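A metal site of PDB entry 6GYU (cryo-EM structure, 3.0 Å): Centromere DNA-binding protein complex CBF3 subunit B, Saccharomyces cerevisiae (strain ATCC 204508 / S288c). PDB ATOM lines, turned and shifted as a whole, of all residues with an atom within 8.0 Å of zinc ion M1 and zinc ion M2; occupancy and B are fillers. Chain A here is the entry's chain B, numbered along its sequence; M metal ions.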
ATOM      1  N   SER A  10      11.054  -7.177  -9.641  1.00  0.00           N
ATOM      2  CA  SER A  10      11.630  -6.100 -10.422  1.00  0.00           C
ATOM      3  C   SER A  10      11.285  -4.756  -9.793  1.00  0.00           C
ATOM      4  O   SER A  10      10.334  -4.636  -9.011  1.00  0.00           O
ATOM      5  CB  SER A  10      11.139  -6.146 -11.865  1.00  0.00           C
ATOM      6  OG  SER A  10       9.756  -5.871 -11.937  1.00  0.00           O
ATOM      7  N   HIS A  12      10.954  -1.454 -11.550  1.00  0.00           N
ATOM      8  CA  HIS A  12       9.967  -0.792 -12.371  1.00  0.00           C
ATOM      9  C   HIS A  12       8.976  -1.815 -12.928  1.00  0.00           C
ATOM     10  O   HIS A  12       9.273  -3.003 -13.021  1.00  0.00           O
ATOM     11  CB  HIS A  12      10.664  -0.051 -13.516  1.00  0.00           C
ATOM     12  CG  HIS A  12      11.524  -0.937 -14.356  1.00  0.00           C
ATOM     13  ND1 HIS A  12      12.820  -1.266 -14.003  1.00  0.00           N
ATOM     14  CD2 HIS A  12      11.280  -1.593 -15.520  1.00  0.00           C
ATOM     15  CE1 HIS A  12      13.335  -2.062 -14.922  1.00  0.00           C
ATOM     16  NE2 HIS A  12      12.418  -2.272 -15.850  1.00  0.00           N
ATOM     17  N   PRO A  13       7.761  -1.366 -13.279  1.00  0.00           N
ATOM     18  CA  PRO A  13       6.875  -2.225 -14.077  1.00  0.00           C
ATOM     19  C   PRO A  13       7.474  -2.493 -15.440  1.00  0.00           C
ATOM     20  O   PRO A  13       8.200  -1.668 -15.999  1.00  0.00           O
ATOM     21  CB  PRO A  13       5.588  -1.399 -14.180  1.00  0.00           C
ATOM     22  CG  PRO A  13       5.622  -0.509 -12.993  1.00  0.00           C
ATOM     23  CD  PRO A  13       7.073  -0.166 -12.788  1.00  0.00           C
ATOM     24  N   CYS A  14       7.165  -3.678 -15.980  1.00  0.00           N
ATOM     25  CA  CYS A  14       7.818  -4.154 -17.188  1.00  0.00           C
ATOM     26  C   CYS A  14       7.358  -3.363 -18.409  1.00  0.00           C
ATOM     27  O   CYS A  14       6.368  -2.620 -18.378  1.00  0.00           O
ATOM     28  CB  CYS A  14       7.543  -5.643 -17.403  1.00  0.00           C
ATOM     29  SG  CYS A  14       5.839  -6.012 -17.861  1.00  0.00           S
ATOM     30  N   SER A  15       8.111  -3.529 -19.500  1.00  0.00           N
ATOM     31  CA  SER A  15       7.834  -2.786 -20.721  1.00  0.00           C
ATOM     32  C   SER A  15       6.550  -3.251 -21.389  1.00  0.00           C
ATOM     33  O   SER A  15       5.907  -2.467 -22.094  1.00  0.00           O
ATOM     34  CB  SER A  15       9.011  -2.932 -21.689  1.00  0.00           C
ATOM     35  OG  SER A  15       9.165  -4.275 -22.100  1.00  0.00           O
ATOM     36  N   VAL A  16       6.155  -4.504 -21.182  1.00  0.00           N
ATOM     37  CA  VAL A  16       4.947  -5.030 -21.810  1.00  0.00           C
ATOM     38  C   VAL A  16       3.704  -4.443 -21.165  1.00  0.00           C
ATOM     39  O   VAL A  16       2.765  -4.040 -21.862  1.00  0.00           O
ATOM     40  CB  VAL A  16       4.960  -6.568 -21.753  1.00  0.00           C
ATOM     41  CG1 VAL A  16       3.680  -7.134 -22.353  1.00  0.00           C
ATOM     42  CG2 VAL A  16       6.177  -7.112 -22.473  1.00  0.00           C
ATOM     43  N   CYS A  17       3.668  -4.360 -19.825  1.00  0.00           N
ATOM     44  CA  CYS A  17       2.515  -3.807 -19.143  1.00  0.00           C
ATOM     45  C   CYS A  17       2.402  -2.285 -19.288  1.00  0.00           C
ATOM     46  O   CYS A  17       1.309  -1.747 -19.099  1.00  0.00           O
ATOM     47  CB  CYS A  17       2.541  -4.186 -17.667  1.00  0.00           C
ATOM     48  SG  CYS A  17       2.234  -5.936 -17.363  1.00  0.00           S
ATOM     49  N   THR A  18       3.492  -1.602 -19.628  1.00  0.00           N
ATOM     50  CA  THR A  18       3.400  -0.198 -20.010  1.00  0.00           C
ATOM     51  C   THR A  18       3.021  -0.019 -21.478  1.00  0.00           C
ATOM     52  O   THR A  18       2.439   1.003 -21.830  1.00  0.00           O
ATOM     53  CB  THR A  18       4.727   0.519 -19.740  1.00  0.00           C
ATOM     54  OG1 THR A  18       5.780  -0.102 -20.480  1.00  0.00           O
ATOM     55  CG2 THR A  18       5.057   0.468 -18.256  1.00  0.00           C
ATOM     56  N   ARG A  20       0.787  -1.898 -22.756  1.00  0.00           N
ATOM     57  CA  ARG A  20      -0.617  -2.275 -22.736  1.00  0.00           C
ATOM     58  C   ARG A  20      -1.434  -1.454 -21.744  1.00  0.00           C
ATOM     59  O   ARG A  20      -2.672  -1.473 -21.811  1.00  0.00           O
ATOM     60  CB  ARG A  20      -0.717  -3.783 -22.419  1.00  0.00           C
ATOM     61  CG  ARG A  20      -2.045  -4.489 -22.625  1.00  0.00           C
ATOM     62  CD  ARG A  20      -1.840  -5.973 -22.474  1.00  0.00           C
ATOM     63  NE  ARG A  20      -1.353  -6.311 -21.133  1.00  0.00           N
ATOM     64  CZ  ARG A  20      -0.813  -7.479 -20.815  1.00  0.00           C
ATOM     65  NH1 ARG A  20      -0.663  -8.413 -21.732  1.00  0.00           N
ATOM     66  NH2 ARG A  20      -0.388  -7.698 -19.579  1.00  0.00           N
ATOM     67  N   VAL A  22      -1.849  -1.623 -18.379  1.00  0.00           N
ATOM     68  CA  VAL A  22      -2.567  -2.383 -17.375  1.00  0.00           C
ATOM     69  C   VAL A  22      -1.752  -2.387 -16.094  1.00  0.00           C
ATOM     70  O   VAL A  22      -0.667  -1.798 -16.021  1.00  0.00           O
ATOM     71  CB  VAL A  22      -2.870  -3.820 -17.830  1.00  0.00           C
ATOM     72  CG1 VAL A  22      -3.774  -3.813 -19.055  1.00  0.00           C
ATOM     73  CG2 VAL A  22      -1.585  -4.570 -18.118  1.00  0.00           C
ATOM     74  N   LYS A  23      -2.280  -3.043 -15.066  1.00  0.00           N
ATOM     75  CA  LYS A  23      -1.531  -3.240 -13.845  1.00  0.00           C
ATOM     76  C   LYS A  23      -0.392  -4.221 -14.079  1.00  0.00           C
ATOM     77  O   LYS A  23      -0.482  -5.088 -14.950  1.00  0.00           O
ATOM     78  CB  LYS A  23      -2.456  -3.725 -12.714  1.00  0.00           C
ATOM     79  CG  LYS A  23      -3.119  -5.086 -12.924  1.00  0.00           C
ATOM     80  CD  LYS A  23      -2.415  -6.222 -12.183  1.00  0.00           C
ATOM     81  CE  LYS A  23      -3.130  -7.554 -12.367  1.00  0.00           C
ATOM     82  NZ  LYS A  23      -2.409  -8.663 -11.692  1.00  0.00           N
ATOM     83  N   CYS A  24       0.673  -4.086 -13.298  1.00  0.00           N
ATOM     84  CA  CYS A  24       1.830  -4.967 -13.410  1.00  0.00           C
ATOM     85  C   CYS A  24       1.952  -5.788 -12.139  1.00  0.00           C
ATOM     86  O   CYS A  24       2.169  -5.240 -11.052  1.00  0.00           O
ATOM     87  CB  CYS A  24       3.098  -4.167 -13.661  1.00  0.00           C
ATOM     88  SG  CYS A  24       4.581  -5.179 -13.886  1.00  0.00           S
ATOM     89  N   ASP A  25       1.810  -7.103 -12.271  1.00  0.00           N
ATOM     90  CA  ASP A  25       2.177  -8.013 -11.204  1.00  0.00           C
ATOM     91  C   ASP A  25       3.695  -8.056 -11.153  1.00  0.00           C
ATOM     92  O   ASP A  25       4.322  -8.905 -11.793  1.00  0.00           O
ATOM     93  CB  ASP A  25       1.597  -9.406 -11.437  1.00  0.00           C
ATOM     94  CG  ASP A  25       1.909 -10.368 -10.315  1.00  0.00           C
ATOM     95  OD1 ASP A  25       1.322 -10.227  -9.218  1.00  0.00           O
ATOM     96  OD2 ASP A  25       2.730 -11.281 -10.523  1.00  0.00           O
ATOM     97  N   ARG A  26       4.286  -7.133 -10.396  1.00  0.00           N
ATOM     98  CA  ARG A  26       5.679  -6.725 -10.589  1.00  0.00           C
ATOM     99  C   ARG A  26       6.648  -7.803 -10.095  1.00  0.00           C
ATOM    100  O   ARG A  26       7.316  -7.626  -9.069  1.00  0.00           O
ATOM    101  CB  ARG A  26       5.912  -5.396  -9.869  1.00  0.00           C
ATOM    102  CG  ARG A  26       7.180  -4.649 -10.246  1.00  0.00           C
ATOM    103  CD  ARG A  26       7.303  -3.383  -9.436  1.00  0.00           C
ATOM    104  NE  ARG A  26       6.259  -2.423  -9.757  1.00  0.00           N
ATOM    105  CZ  ARG A  26       6.043  -1.310  -9.065  1.00  0.00           C
ATOM    106  NH1 ARG A  26       5.073  -0.484  -9.421  1.00  0.00           N
ATOM    107  NH2 ARG A  26       6.806  -1.036  -8.011  1.00  0.00           N
ATOM    108  N   MET A  27       6.703  -8.912 -10.804  1.00  0.00           N
ATOM    109  CA  MET A  27       7.641  -9.998 -10.531  1.00  0.00           C
ATOM    110  C   MET A  27       8.699 -10.007 -11.628  1.00  0.00           C
ATOM    111  O   MET A  27       8.770  -9.108 -12.473  1.00  0.00           O
ATOM    112  CB  MET A  27       6.918 -11.346 -10.474  1.00  0.00           C
ATOM    113  CG  MET A  27       5.837 -11.486  -9.416  1.00  0.00           C
ATOM    114  SD  MET A  27       6.335 -11.164  -7.718  1.00  0.00           S
ATOM    115  CE  MET A  27       5.367  -9.711  -7.352  1.00  0.00           C
ATOM    116  N   ILE A  28       9.539 -11.031 -11.595  1.00  0.00           N
ATOM    117  CA  ILE A  28      10.389 -11.394 -12.719  1.00  0.00           C
ATOM    118  C   ILE A  28      10.049 -12.825 -13.122  1.00  0.00           C
ATOM    119  O   ILE A  28      10.284 -13.740 -12.341  1.00  0.00           O
ATOM    120  CB  ILE A  28      11.889 -11.249 -12.419  1.00  0.00           C
ATOM    121  CG1 ILE A  28      12.252  -9.764 -12.300  1.00  0.00           C
ATOM    122  CG2 ILE A  28      12.732 -11.883 -13.496  1.00  0.00           C
ATOM    123  CD1 ILE A  28      13.702  -9.500 -11.942  1.00  0.00           C
ATOM    124  N   PRO A  29       9.466 -13.057 -14.307  1.00  0.00           N
ATOM    125  CA  PRO A  29       9.150 -12.011 -15.301  1.00  0.00           C
ATOM    126  C   PRO A  29       7.863 -11.201 -15.052  1.00  0.00           C
ATOM    127  O   PRO A  29       7.967  -9.983 -15.119  1.00  0.00           O
ATOM    128  CB  PRO A  29       9.004 -12.815 -16.600  1.00  0.00           C
ATOM    129  CG  PRO A  29       8.593 -14.174 -16.163  1.00  0.00           C
ATOM    130  CD  PRO A  29       9.256 -14.418 -14.847  1.00  0.00           C
ATOM    131  N   CYS A  30       6.765 -11.862 -14.678  1.00  0.00           N
ATOM    132  CA  CYS A  30       5.459 -11.300 -14.327  1.00  0.00           C
ATOM    133  C   CYS A  30       4.511 -12.418 -13.954  1.00  0.00           C
ATOM    134  O   CYS A  30       4.807 -13.597 -14.171  1.00  0.00           O
ATOM    135  CB  CYS A  30       4.804 -10.499 -15.463  1.00  0.00           C
ATOM    136  SG  CYS A  30       5.150  -8.732 -15.602  1.00  0.00           S
ATOM    137  N   GLY A  31       3.356 -12.058 -13.401  1.00  0.00           N
ATOM    138  CA  GLY A  31       2.224 -12.972 -13.428  1.00  0.00           C
ATOM    139  C   GLY A  31       1.329 -12.692 -14.618  1.00  0.00           C
ATOM    140  O   GLY A  31       0.574 -13.577 -15.038  1.00  0.00           O
ATOM    141  N   ASN A  32       1.419 -11.490 -15.179  1.00  0.00           N
ATOM    142  CA  ASN A  32       0.532 -11.038 -16.242  1.00  0.00           C
ATOM    143  C   ASN A  32       1.115 -11.314 -17.621  1.00  0.00           C
ATOM    144  O   ASN A  32       0.374 -11.429 -18.605  1.00  0.00           O
ATOM    145  CB  ASN A  32       0.253  -9.548 -16.062  1.00  0.00           C
ATOM    146  CG  ASN A  32      -1.005  -9.088 -16.764  1.00  0.00           C
ATOM    147  OD1 ASN A  32      -1.709  -9.871 -17.402  1.00  0.00           O
ATOM    148  ND2 ASN A  32      -1.310  -7.797 -16.644  1.00  0.00           N
ATOM    149  N   CYS A  33       2.445 -11.442 -17.708  1.00  0.00           N
ATOM    150  CA  CYS A  33       3.078 -11.814 -18.969  1.00  0.00           C
ATOM    151  C   CYS A  33       3.321 -13.317 -19.046  1.00  0.00           C
ATOM    152  O   CYS A  33       3.330 -13.879 -20.143  1.00  0.00           O
ATOM    153  CB  CYS A  33       4.390 -11.061 -19.151  1.00  0.00           C
ATOM    154  SG  CYS A  33       4.190  -9.274 -19.337  1.00  0.00           S
ATOM    155  N   ARG A  34       3.517 -13.969 -17.904  1.00  0.00           N
ATOM    156  CA  ARG A  34       3.601 -15.427 -17.864  1.00  0.00           C
ATOM    157  C   ARG A  34       2.231 -16.056 -18.109  1.00  0.00           C
ATOM    158  O   ARG A  34       2.162 -17.214 -18.558  1.00  0.00           O
ATOM    159  CB  ARG A  34       4.189 -15.861 -16.523  1.00  0.00           C
ATOM    160  CG  ARG A  34       4.504 -17.331 -16.359  1.00  0.00           C
ATOM    161  CD  ARG A  34       5.206 -17.550 -15.032  1.00  0.00           C
ATOM    162  NE  ARG A  34       5.559 -18.943 -14.773  1.00  0.00           N
ATOM    163  CZ  ARG A  34       4.776 -19.789 -14.106  1.00  0.00           C
ATOM    164  NH1 ARG A  34       3.616 -19.379 -13.633  1.00  0.00           N
ATOM    165  NH2 ARG A  34       5.173 -21.039 -13.918  1.00  0.00           N
ATOM    166  N   GLN A  38       4.454 -14.965 -22.532  1.00  0.00           N
ATOM    167  CA  GLN A  38       5.446 -13.975 -22.941  1.00  0.00           C
ATOM    168  C   GLN A  38       6.632 -13.957 -21.999  1.00  0.00           C
ATOM    169  O   GLN A  38       7.112 -12.881 -21.613  1.00  0.00           O
ATOM    170  CB  GLN A  38       4.804 -12.598 -23.060  1.00  0.00           C
ATOM    171  CG  GLN A  38       3.796 -12.493 -24.182  1.00  0.00           C
ATOM    172  CD  GLN A  38       3.150 -11.134 -24.268  1.00  0.00           C
ATOM    173  OE1 GLN A  38       3.407 -10.272 -23.433  1.00  0.00           O
ATOM    174  NE2 GLN A  38       2.324 -10.923 -25.282  1.00  0.00           N
ATOM    175  N   ASP A  39       7.081 -15.141 -21.584  1.00  0.00           N
ATOM    176  CA  ASP A  39       8.183 -15.282 -20.634  1.00  0.00           C
ATOM    177  C   ASP A  39       9.476 -14.682 -21.178  1.00  0.00           C
ATOM    178  O   ASP A  39      10.121 -13.860 -20.512  1.00  0.00           O
ATOM    179  CB  ASP A  39       8.384 -16.764 -20.305  1.00  0.00           C
ATOM    180  CG  ASP A  39       9.482 -16.995 -19.284  1.00  0.00           C
ATOM    181  OD1 ASP A  39       9.251 -16.763 -18.084  1.00  0.00           O
ATOM    182  OD2 ASP A  39      10.596 -17.408 -19.692  1.00  0.00           O
ATOM    183  N   GLU A  41       9.970 -12.593 -23.608  1.00  0.00           N
ATOM    184  CA  GLU A  41       9.862 -11.207 -24.038  1.00  0.00           C
ATOM    185  C   GLU A  41       9.769 -10.228 -22.866  1.00  0.00           C
ATOM    186  O   GLU A  41       9.397  -9.073 -23.064  1.00  0.00           O
ATOM    187  CB  GLU A  41       8.658 -11.030 -24.959  1.00  0.00           C
ATOM    188  CG  GLU A  41       8.767 -11.781 -26.275  1.00  0.00           C
ATOM    189  CD  GLU A  41       9.859 -11.226 -27.180  1.00  0.00           C
ATOM    190  OE1 GLU A  41      10.099  -9.998 -27.138  1.00  0.00           O
ATOM    191  OE2 GLU A  41      10.478 -12.015 -27.920  1.00  0.00           O
ATOM    192  N   CYS A  42      10.091 -10.675 -21.649  1.00  0.00           N
ATOM    193  CA  CYS A  42      10.032  -9.812 -20.479  1.00  0.00           C
ATOM    194  C   CYS A  42      11.327  -9.933 -19.674  1.00  0.00           C
ATOM    195  O   CYS A  42      11.700  -9.019 -18.942  1.00  0.00           O
ATOM    196  CB  CYS A  42       8.820 -10.177 -19.619  1.00  0.00           C
ATOM    197  SG  CYS A  42       8.538  -9.106 -18.195  1.00  0.00           S
ATOM    198  N   MET A  43      12.023 -11.070 -19.833  1.00  0.00           N
ATOM    199  CA  MET A  43      13.262 -11.295 -19.099  1.00  0.00           C
ATOM    200  C   MET A  43      14.398 -10.418 -19.602  1.00  0.00           C
ATOM    201  O   MET A  43      15.319 -10.100 -18.839  1.00  0.00           O
ATOM    202  CB  MET A  43      13.669 -12.762 -19.209  1.00  0.00           C
ATOM    203  CG  MET A  43      12.731 -13.747 -18.535  1.00  0.00           C
ATOM    204  SD  MET A  43      12.621 -13.485 -16.766  1.00  0.00           S
ATOM    205  CE  MET A  43      14.270 -13.986 -16.255  1.00  0.00           C
HETATM  206 ZN    ZN M   1       6.113  -8.551 -17.902  1.00  0.00          ZN
HETATM  207 ZN    ZN M   2       4.201  -6.494 -15.976  1.00  0.00          ZN
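O of Cys 17 sits at hydrogen-bond distance from N of Val 22, 3.2 Å away.
The backbone carbonyl oxygen of Cys 33 lies within hydrogen-bond range of the backbone NH of Gln 38, at 2.9 Å.
The backbone carbonyl oxygen (O) of Cys 14 lies within hydrogen-bond range of the side-chain hydroxyl (OG1) of Thr 18.
The side-chain sulfur of Cys 42 lies close to the backbone carbonyl oxygen of Pro 29 (3.2 Å).
N of Val 16 lies close to SG of Cys 14, at 3.7 Å.
The backbone carbonyl oxygen of Lys 23 lies close to the side-chain sulfur of Cys 17 (3.7 Å).
O of Pro 29 touches zinc ion M1, 3.6 Å away.
SG of Cys 30 binds zinc ion M1.
SG of Cys 42 is bound to zinc ion M1, at 2.5 Å.
SG of Cys 33 binds zinc ion M1, 2.5 Å away.
The side-chain sulfur (SG) of Cys 14 binds zinc ion M1, 2.6 Å away.
Zinc ion M1 has four donor atoms within binding distance.
The nearest printed residue that does not touch zinc ion M2 is Cys 33 (4.4 Å).
Zinc ion M2 is bound by SG of Cys 30 (2.5 Å), SG of Cys 17 (2.5 Å), SG of Cys 24 (2.5 Å) and SG of Cys 14 (2.5 Å).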
